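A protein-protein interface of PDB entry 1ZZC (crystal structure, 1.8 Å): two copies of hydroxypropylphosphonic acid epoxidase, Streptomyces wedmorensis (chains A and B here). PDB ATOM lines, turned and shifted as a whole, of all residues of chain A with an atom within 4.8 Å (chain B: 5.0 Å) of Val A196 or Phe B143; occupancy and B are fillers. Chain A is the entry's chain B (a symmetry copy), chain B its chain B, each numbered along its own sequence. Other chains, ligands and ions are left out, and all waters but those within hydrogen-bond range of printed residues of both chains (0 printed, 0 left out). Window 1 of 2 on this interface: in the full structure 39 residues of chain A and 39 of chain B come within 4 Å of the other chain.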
ATOM      1  N   LEU A 108       8.160 -17.999 -12.264  1.00  0.00           N
ATOM      2  CA  LEU A 108       8.872 -17.948 -13.525  1.00  0.00           C
ATOM      3  C   LEU A 108       8.980 -16.485 -13.970  1.00  0.00           C
ATOM      4  O   LEU A 108       8.545 -15.584 -13.257  1.00  0.00           O
ATOM      5  CB  LEU A 108       8.147 -18.804 -14.579  1.00  0.00           C
ATOM      6  CG  LEU A 108       8.001 -20.268 -14.141  1.00  0.00           C
ATOM      7  CD1 LEU A 108       7.095 -21.028 -15.134  1.00  0.00           C
ATOM      8  CD2 LEU A 108       9.418 -20.919 -14.077  1.00  0.00           C
ATOM      9  N   VAL A 109       9.558 -16.265 -15.139  1.00  0.00           N
ATOM     10  CA  VAL A 109       9.796 -14.913 -15.654  1.00  0.00           C
ATOM     11  C   VAL A 109       8.560 -14.011 -15.728  1.00  0.00           C
ATOM     12  O   VAL A 109       7.477 -14.460 -16.077  1.00  0.00           O
ATOM     13  CB  VAL A 109      10.490 -14.984 -17.063  1.00  0.00           C
ATOM     14  CG1 VAL A 109       9.465 -15.382 -18.160  1.00  0.00           C
ATOM     15  CG2 VAL A 109      11.147 -13.643 -17.405  1.00  0.00           C
ATOM     16  N   LEU A 117       0.957 -10.975 -16.766  1.00  0.00           N
ATOM     17  CA  LEU A 117       1.554 -12.281 -16.989  1.00  0.00           C
ATOM     18  C   LEU A 117       2.259 -12.740 -15.723  1.00  0.00           C
ATOM     19  O   LEU A 117       3.244 -12.139 -15.297  1.00  0.00           O
ATOM     20  CB  LEU A 117       2.574 -12.234 -18.139  1.00  0.00           C
ATOM     21  CG  LEU A 117       3.455 -13.487 -18.325  1.00  0.00           C
ATOM     22  CD1 LEU A 117       2.593 -14.698 -18.660  1.00  0.00           C
ATOM     23  CD2 LEU A 117       4.473 -13.258 -19.456  1.00  0.00           C
ATOM     24  N   VAL A 118       1.756 -13.813 -15.132  1.00  0.00           N
ATOM     25  CA  VAL A 118       2.369 -14.343 -13.923  1.00  0.00           C
ATOM     26  C   VAL A 118       2.425 -15.852 -14.102  1.00  0.00           C
ATOM     27  O   VAL A 118       1.444 -16.527 -13.876  1.00  0.00           O
ATOM     28  CB  VAL A 118       1.530 -14.003 -12.668  1.00  0.00           C
ATOM     29  CG1 VAL A 118       2.235 -14.578 -11.401  1.00  0.00           C
ATOM     30  CG2 VAL A 118       1.366 -12.475 -12.536  1.00  0.00           C
ATOM     31  N   PRO A 119       3.553 -16.378 -14.598  1.00  0.00           N
ATOM     32  CA  PRO A 119       3.684 -17.830 -14.795  1.00  0.00           C
ATOM     33  C   PRO A 119       4.389 -18.441 -13.581  1.00  0.00           C
ATOM     34  O   PRO A 119       5.322 -17.853 -13.043  1.00  0.00           O
ATOM     35  CB  PRO A 119       4.492 -17.946 -16.083  1.00  0.00           C
ATOM     36  CG  PRO A 119       5.348 -16.735 -16.099  1.00  0.00           C
ATOM     37  CD  PRO A 119       4.648 -15.643 -15.251  1.00  0.00           C
ATOM     38  N   ASN A 141      -7.522 -14.535 -17.388  1.00  0.00           N
ATOM     39  CA  ASN A 141      -7.555 -15.935 -17.794  1.00  0.00           C
ATOM     40  C   ASN A 141      -6.336 -16.702 -17.295  1.00  0.00           C
ATOM     41  O   ASN A 141      -5.356 -16.115 -16.842  1.00  0.00           O
ATOM     42  CB  ASN A 141      -7.614 -16.037 -19.324  1.00  0.00           C
ATOM     43  CG  ASN A 141      -8.881 -15.431 -19.895  1.00  0.00           C
ATOM     44  OD1 ASN A 141      -9.954 -15.547 -19.298  1.00  0.00           O
ATOM     45  ND2 ASN A 141      -8.770 -14.808 -21.062  1.00  0.00           N
ATOM     46  N   GLU A 142      -6.397 -18.022 -17.404  1.00  0.00           N
ATOM     47  CA  GLU A 142      -5.286 -18.859 -16.958  1.00  0.00           C
ATOM     48  C   GLU A 142      -5.146 -20.110 -17.823  1.00  0.00           C
ATOM     49  O   GLU A 142      -6.132 -20.749 -18.151  1.00  0.00           O
ATOM     50  CB  GLU A 142      -5.505 -19.280 -15.504  1.00  0.00           C
ATOM     51  CG  GLU A 142      -4.275 -19.927 -14.870  1.00  0.00           C
ATOM     52  CD  GLU A 142      -4.555 -20.418 -13.464  1.00  0.00           C
ATOM     53  OE1 GLU A 142      -5.347 -19.772 -12.758  1.00  0.00           O
ATOM     54  OE2 GLU A 142      -3.982 -21.439 -13.052  1.00  0.00           O
ATOM     55  N   PHE A 143      -3.907 -20.445 -18.171  1.00  0.00           N
ATOM     56  CA  PHE A 143      -3.587 -21.636 -18.953  1.00  0.00           C
ATOM     57  C   PHE A 143      -2.730 -22.514 -18.036  1.00  0.00           C
ATOM     58  O   PHE A 143      -1.868 -21.991 -17.346  1.00  0.00           O
ATOM     59  CB  PHE A 143      -2.751 -21.264 -20.173  1.00  0.00           C
ATOM     60  CG  PHE A 143      -2.016 -22.419 -20.771  1.00  0.00           C
ATOM     61  CD1 PHE A 143      -2.687 -23.359 -21.555  1.00  0.00           C
ATOM     62  CD2 PHE A 143      -0.660 -22.609 -20.504  1.00  0.00           C
ATOM     63  CE1 PHE A 143      -2.008 -24.468 -22.062  1.00  0.00           C
ATOM     64  CE2 PHE A 143       0.018 -23.711 -21.006  1.00  0.00           C
ATOM     65  CZ  PHE A 143      -0.659 -24.649 -21.784  1.00  0.00           C
ATOM     66  N   ILE A 194       2.318 -26.192 -14.478  1.00  0.00           N
ATOM     67  CA  ILE A 194       2.820 -24.870 -14.870  1.00  0.00           C
ATOM     68  C   ILE A 194       1.500 -24.101 -14.999  1.00  0.00           C
ATOM     69  O   ILE A 194       0.588 -24.561 -15.695  1.00  0.00           O
ATOM     70  CB  ILE A 194       3.492 -24.832 -16.242  1.00  0.00           C
ATOM     71  CG1 ILE A 194       4.765 -25.669 -16.216  1.00  0.00           C
ATOM     72  CG2 ILE A 194       3.835 -23.357 -16.595  1.00  0.00           C
ATOM     73  CD1 ILE A 194       5.431 -25.792 -17.549  1.00  0.00           C
ATOM     74  N   ALA A 195       1.368 -22.988 -14.285  1.00  0.00           N
ATOM     75  CA  ALA A 195       0.158 -22.172 -14.369  1.00  0.00           C
ATOM     76  C   ALA A 195       0.592 -20.831 -14.939  1.00  0.00           C
ATOM     77  O   ALA A 195       1.526 -20.200 -14.427  1.00  0.00           O
ATOM     78  CB  ALA A 195      -0.449 -21.965 -13.017  1.00  0.00           C
ATOM     79  N   VAL A 196      -0.067 -20.418 -16.011  1.00  0.00           N
ATOM     80  CA  VAL A 196       0.248 -19.150 -16.653  1.00  0.00           C
ATOM     81  C   VAL A 196      -0.989 -18.257 -16.590  1.00  0.00           C
ATOM     82  O   VAL A 196      -1.963 -18.480 -17.300  1.00  0.00           O
ATOM     83  CB  VAL A 196       0.634 -19.347 -18.137  1.00  0.00           C
ATOM     84  CG1 VAL A 196       1.095 -18.010 -18.736  1.00  0.00           C
ATOM     85  CG2 VAL A 196       1.740 -20.421 -18.252  1.00  0.00           C
ATOM     86  N   ASN A 197      -0.963 -17.280 -15.697  1.00  0.00           N
ATOM     87  CA  ASN A 197      -2.072 -16.355 -15.587  1.00  0.00           C
ATOM     88  C   ASN A 197      -1.714 -15.198 -16.521  1.00  0.00           C
ATOM     89  O   ASN A 197      -0.544 -14.824 -16.630  1.00  0.00           O
ATOM     90  CB  ASN A 197      -2.234 -15.908 -14.135  1.00  0.00           C
ATOM     91  CG  ASN A 197      -3.024 -16.925 -13.318  1.00  0.00           C
ATOM     92  OD1 ASN A 197      -4.260 -16.838 -13.213  1.00  0.00           O
ATOM     93  ND2 ASN A 197      -2.328 -17.915 -12.772  1.00  0.00           N
ATOM     94  N   PHE A 198      -2.706 -14.687 -17.241  1.00  0.00           N
ATOM     95  CA  PHE A 198      -2.457 -13.609 -18.191  1.00  0.00           C
ATOM     96  C   PHE A 198      -3.734 -12.804 -18.447  1.00  0.00           C
ATOM     97  O   PHE A 198      -4.686 -13.017 -17.662  1.00  0.00           O
ATOM     98  CB  PHE A 198      -1.928 -14.193 -19.523  1.00  0.00           C
ATOM     99  CG  PHE A 198      -2.918 -15.084 -20.237  1.00  0.00           C
ATOM    100  CD1 PHE A 198      -3.116 -16.402 -19.835  1.00  0.00           C
ATOM    101  CD2 PHE A 198      -3.651 -14.593 -21.318  1.00  0.00           C
ATOM    102  CE1 PHE A 198      -4.024 -17.230 -20.494  1.00  0.00           C
ATOM    103  CE2 PHE A 198      -4.569 -15.402 -21.997  1.00  0.00           C
ATOM    104  CZ  PHE A 198      -4.763 -16.729 -21.587  1.00  0.00           C
ATOM    105  N   ASN B 141       2.214 -11.276 -27.615  1.00  0.00           N
ATOM    106  CA  ASN B 141       3.321 -11.689 -26.763  1.00  0.00           C
ATOM    107  C   ASN B 141       3.458 -13.206 -26.700  1.00  0.00           C
ATOM    108  O   ASN B 141       2.568 -13.942 -27.117  1.00  0.00           O
ATOM    109  CB  ASN B 141       3.122 -11.148 -25.342  1.00  0.00           C
ATOM    110  CG  ASN B 141       3.131  -9.633 -25.292  1.00  0.00           C
ATOM    111  OD1 ASN B 141       3.890  -8.989 -26.019  1.00  0.00           O
ATOM    112  ND2 ASN B 141       2.310  -9.062 -24.418  1.00  0.00           N
ATOM    113  N   GLU B 142       4.575 -13.665 -26.153  1.00  0.00           N
ATOM    114  CA  GLU B 142       4.813 -15.103 -26.039  1.00  0.00           C
ATOM    115  C   GLU B 142       5.614 -15.439 -24.785  1.00  0.00           C
ATOM    116  O   GLU B 142       6.579 -14.763 -24.465  1.00  0.00           O
ATOM    117  CB  GLU B 142       5.577 -15.600 -27.268  1.00  0.00           C
ATOM    118  CG  GLU B 142       5.634 -17.123 -27.369  1.00  0.00           C
ATOM    119  CD  GLU B 142       6.477 -17.582 -28.541  1.00  0.00           C
ATOM    120  OE1 GLU B 142       6.479 -16.894 -29.575  1.00  0.00           O
ATOM    121  OE2 GLU B 142       7.133 -18.631 -28.443  1.00  0.00           O
ATOM    122  N   PHE B 143       5.203 -16.499 -24.094  1.00  0.00           N
ATOM    123  CA  PHE B 143       5.880 -16.990 -22.897  1.00  0.00           C
ATOM    124  C   PHE B 143       6.379 -18.394 -23.254  1.00  0.00           C
ATOM    125  O   PHE B 143       5.649 -19.141 -23.888  1.00  0.00           O
ATOM    126  CB  PHE B 143       4.897 -17.113 -21.739  1.00  0.00           C
ATOM    127  CG  PHE B 143       5.375 -18.002 -20.638  1.00  0.00           C
ATOM    128  CD1 PHE B 143       6.339 -17.557 -19.733  1.00  0.00           C
ATOM    129  CD2 PHE B 143       4.909 -19.313 -20.536  1.00  0.00           C
ATOM    130  CE1 PHE B 143       6.825 -18.412 -18.742  1.00  0.00           C
ATOM    131  CE2 PHE B 143       5.391 -20.166 -19.553  1.00  0.00           C
ATOM    132  CZ  PHE B 143       6.357 -19.717 -18.654  1.00  0.00           C
ATOM    133  N   LEU B 144       7.608 -18.727 -22.857  1.00  0.00           N
ATOM    134  CA  LEU B 144       8.172 -20.040 -23.145  1.00  0.00           C
ATOM    135  C   LEU B 144       8.810 -20.628 -21.908  1.00  0.00           C
ATOM    136  O   LEU B 144       9.297 -19.891 -21.044  1.00  0.00           O
ATOM    137  CB  LEU B 144       9.224 -19.941 -24.247  1.00  0.00           C
ATOM    138  CG  LEU B 144       8.729 -19.440 -25.609  1.00  0.00           C
ATOM    139  CD1 LEU B 144       9.168 -17.960 -25.807  1.00  0.00           C
ATOM    140  CD2 LEU B 144       9.334 -20.306 -26.704  1.00  0.00           C
ATOM    141  N   PHE B 145       8.814 -21.959 -21.831  1.00  0.00           N
ATOM    142  CA  PHE B 145       9.397 -22.701 -20.716  1.00  0.00           C
ATOM    143  C   PHE B 145      10.172 -23.874 -21.356  1.00  0.00           C
ATOM    144  O   PHE B 145       9.634 -24.554 -22.239  1.00  0.00           O
ATOM    145  CB  PHE B 145       8.269 -23.254 -19.838  1.00  0.00           C
ATOM    146  CG  PHE B 145       8.740 -24.062 -18.661  1.00  0.00           C
ATOM    147  CD1 PHE B 145       9.217 -23.438 -17.517  1.00  0.00           C
ATOM    148  CD2 PHE B 145       8.659 -25.457 -18.686  1.00  0.00           C
ATOM    149  CE1 PHE B 145       9.613 -24.183 -16.395  1.00  0.00           C
ATOM    150  CE2 PHE B 145       9.052 -26.220 -17.571  1.00  0.00           C
ATOM    151  CZ  PHE B 145       9.526 -25.575 -16.425  1.00  0.00           C
ATOM    152  N   SER B 171      12.813 -19.932 -18.371  1.00  0.00           N
ATOM    153  CA  SER B 171      11.599 -19.369 -18.949  1.00  0.00           C
ATOM    154  C   SER B 171      11.968 -18.061 -19.658  1.00  0.00           C
ATOM    155  O   SER B 171      12.952 -17.408 -19.305  1.00  0.00           O
ATOM    156  CB  SER B 171      10.522 -19.137 -17.873  1.00  0.00           C
ATOM    157  OG  SER B 171      10.978 -18.311 -16.806  1.00  0.00           O
ATOM    158  N   MET B 172      11.175 -17.698 -20.656  1.00  0.00           N
ATOM    159  CA  MET B 172      11.424 -16.501 -21.430  1.00  0.00           C
ATOM    160  C   MET B 172      10.133 -15.814 -21.840  1.00  0.00           C
ATOM    161  O   MET B 172       9.073 -16.429 -21.935  1.00  0.00           O
ATOM    162  CB  MET B 172      12.184 -16.838 -22.726  1.00  0.00           C
ATOM    163  CG  MET B 172      13.342 -17.823 -22.566  1.00  0.00           C
ATOM    164  SD  MET B 172      12.815 -19.606 -22.440  1.00  0.00           S
ATOM    165  CE  MET B 172      12.964 -20.129 -24.208  1.00  0.00           C
ATOM    166  N   PHE B 173      10.259 -14.527 -22.130  1.00  0.00           N
ATOM    167  CA  PHE B 173       9.129 -13.742 -22.594  1.00  0.00           C
ATOM    168  C   PHE B 173       9.636 -13.052 -23.840  1.00  0.00           C
ATOM    169  O   PHE B 173      10.754 -12.507 -23.841  1.00  0.00           O
ATOM    170  CB  PHE B 173       8.742 -12.678 -21.571  1.00  0.00           C
ATOM    171  CG  PHE B 173       7.805 -11.646 -22.117  1.00  0.00           C
ATOM    172  CD1 PHE B 173       6.435 -11.865 -22.123  1.00  0.00           C
ATOM    173  CD2 PHE B 173       8.306 -10.446 -22.640  1.00  0.00           C
ATOM    174  CE1 PHE B 173       5.552 -10.901 -22.640  1.00  0.00           C
ATOM    175  CE2 PHE B 173       7.446  -9.485 -23.155  1.00  0.00           C
ATOM    176  CZ  PHE B 173       6.065  -9.712 -23.153  1.00  0.00           C
ATOM    177  N   ILE B 194       7.670 -25.404 -24.182  1.00  0.00           N
ATOM    178  CA  ILE B 194       6.226 -25.139 -24.180  1.00  0.00           C
ATOM    179  C   ILE B 194       6.217 -23.665 -24.603  1.00  0.00           C
ATOM    180  O   ILE B 194       6.916 -22.849 -23.995  1.00  0.00           O
ATOM    181  CB  ILE B 194       5.574 -25.210 -22.800  1.00  0.00           C
ATOM    182  CG1 ILE B 194       5.645 -26.637 -22.269  1.00  0.00           C
ATOM    183  CG2 ILE B 194       4.090 -24.761 -22.920  1.00  0.00           C
ATOM    184  CD1 ILE B 194       5.138 -26.783 -20.870  1.00  0.00           C
ATOM    185  N   ALA B 195       5.496 -23.341 -25.671  1.00  0.00           N
ATOM    186  CA  ALA B 195       5.400 -21.956 -26.128  1.00  0.00           C
ATOM    187  C   ALA B 195       3.938 -21.564 -25.984  1.00  0.00           C
ATOM    188  O   ALA B 195       3.045 -22.263 -26.480  1.00  0.00           O
ATOM    189  CB  ALA B 195       5.810 -21.831 -27.561  1.00  0.00           C
ATOM    190  N   VAL B 196       3.699 -20.465 -25.284  1.00  0.00           N
ATOM    191  CA  VAL B 196       2.344 -19.978 -25.074  1.00  0.00           C
ATOM    192  C   VAL B 196       2.228 -18.589 -25.699  1.00  0.00           C
ATOM    193  O   VAL B 196       2.756 -17.616 -25.173  1.00  0.00           O
ATOM    194  CB  VAL B 196       2.009 -19.868 -23.569  1.00  0.00           C
ATOM    195  CG1 VAL B 196       0.530 -19.490 -23.392  1.00  0.00           C
ATOM    196  CG2 VAL B 196       2.333 -21.204 -22.861  1.00  0.00           C
ATOM    197  N   ASN B 197       1.579 -18.517 -26.850  1.00  0.00           N
ATOM    198  CA  ASN B 197       1.380 -17.238 -27.502  1.00  0.00           C
ATOM    199  C   ASN B 197       0.036 -16.733 -26.977  1.00  0.00           C
ATOM    200  O   ASN B 197      -0.889 -17.521 -26.766  1.00  0.00           O
ATOM    201  CB  ASN B 197       1.386 -17.422 -29.018  1.00  0.00           C
ATOM    202  CG  ASN B 197       2.806 -17.466 -29.575  1.00  0.00           C
ATOM    203  OD1 ASN B 197       3.374 -16.428 -29.957  1.00  0.00           O
ATOM    204  ND2 ASN B 197       3.400 -18.653 -29.585  1.00  0.00           N
ATOM    205  N   PHE B 198      -0.044 -15.436 -26.701  1.00  0.00           N
ATOM    206  CA  PHE B 198      -1.271 -14.866 -26.156  1.00  0.00           C
ATOM    207  C   PHE B 198      -1.360 -13.368 -26.467  1.00  0.00           C
ATOM    208  O   PHE B 198      -0.542 -12.931 -27.308  1.00  0.00           O
ATOM    209  CB  PHE B 198      -1.322 -15.089 -24.627  1.00  0.00           C
ATOM    210  CG  PHE B 198      -0.224 -14.379 -23.868  1.00  0.00           C
ATOM    211  CD1 PHE B 198       1.066 -14.901 -23.817  1.00  0.00           C
ATOM    212  CD2 PHE B 198      -0.491 -13.182 -23.202  1.00  0.00           C
ATOM    213  CE1 PHE B 198       2.081 -14.253 -23.114  1.00  0.00           C
ATOM    214  CE2 PHE B 198       0.508 -12.511 -22.489  1.00  0.00           C
ATOM    215  CZ  PHE B 198       1.804 -13.043 -22.442  1.00  0.00           C
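The backbone NH (N) of Val A109 lies within hydrogen-bond range of the side-chain hydroxyl (OG) of Ser B171 (3.0 Å).
Leu A108 touches Phe B143.
Leu A108 touches Phe B145.
OG of Ser B171 touches CB of Leu A108, at 3.6 Å.
Val A109 touches Met B172 (CG1 to C, 3.8 Å).
CD1 of Phe B173 touches CD2 of Leu A117, at 3.6 Å.
Phe B143 touches Pro A119 (CE1 to CG, 3.5 Å).
CD1 of Ile A194 touches CD2 of Phe B145 (3.4 Å).
CD1 of Ile B194 touches CD1 of Ile A194, 3.5 Å away.
Phe B143 touches Val A196.
Phe B198 touches Phe A198 (CD2 to CD2, 3.9 Å).
Val A196 touches one residue of chain B.
Printed residues of chain A within 4 Å of Phe B143: Leu A108, Pro A119 and Val A196.
Of the printed residues of chain B, Leu A108 touches Phe B143 (3.8 Å), Phe B145 (3.999 Å) and Ser B171 (3.6 Å).
Of the printed residues of chain A, Ile B194 touches Ile A194.
The nearest residue of chain A that does not touch Phe B143 is Val A109 (4.1 Å).
The nearest printed residue of chain B that does not touch Phe A143 is Ile B194 (4.6 Å).
The backbone NH (N) of Val B196 sits at hydrogen-bond distance from the backbone carbonyl oxygen (O) of Phe B143, at 2.7 Å.
The backbone NH of Leu B144 sits at hydrogen-bond distance from the backbone carbonyl oxygen of Met B172, 2.9 Å away.
The backbone carbonyl oxygen (O) of Phe B145 is in hydrogen-bond range of the backbone NH (N) of Ile B194, 2.9 Å away.
The backbone NH (N) of Leu A108 sits at hydrogen-bond distance from the backbone carbonyl oxygen (O) of Pro A119, 2.9 Å away.
The backbone NH (N) of Phe A198 is in hydrogen-bond range of the backbone carbonyl oxygen (O) of Asn A141, 3.0 Å away.
The backbone carbonyl oxygen (O) of Phe A143 lies within hydrogen-bond range of the backbone NH (N) of Val A196 (2.7 Å).
Printed residues of chain B that touch a printed residue of chain A: Phe B143, Phe B145, Ser B171, Met B172, Phe B173, Ile B194, Val B196 and Phe B198.
Hydrophobic or aromatic side chains of chain B that line the printed part of chain A: Phe B143, Phe B145, Phe B173, Ile B194, Val B196 and Phe B198.
Printed residues of chain A that touch a printed residue of chain B: Leu A108, Val A109, Leu A117, Pro A119, Phe A143, Ile A194, Val A196 and Phe A198.
Hydrophobic or aromatic side chains of chain A that line the printed part of chain B: Leu A108, Val A109, Leu A117, Pro A119, Phe A143, Ile A194, Val A196 and Phe A198.
Among the printed residues, no Asp or Glu carboxylate lies within 4 Å of a Lys or Arg side-chain nitrogen of the other chain.
Phe A143 touches Val B196, and with the chains exchanged Val A196 touches Phe B143.
Ile A194 touches its own counterpart, Ile B194.
Phe B198 touches its own counterpart, Phe A198.
Of the 12 pairs that touch across the chains among the printed residues, 4 have their exchanged pair printed and touching as well.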
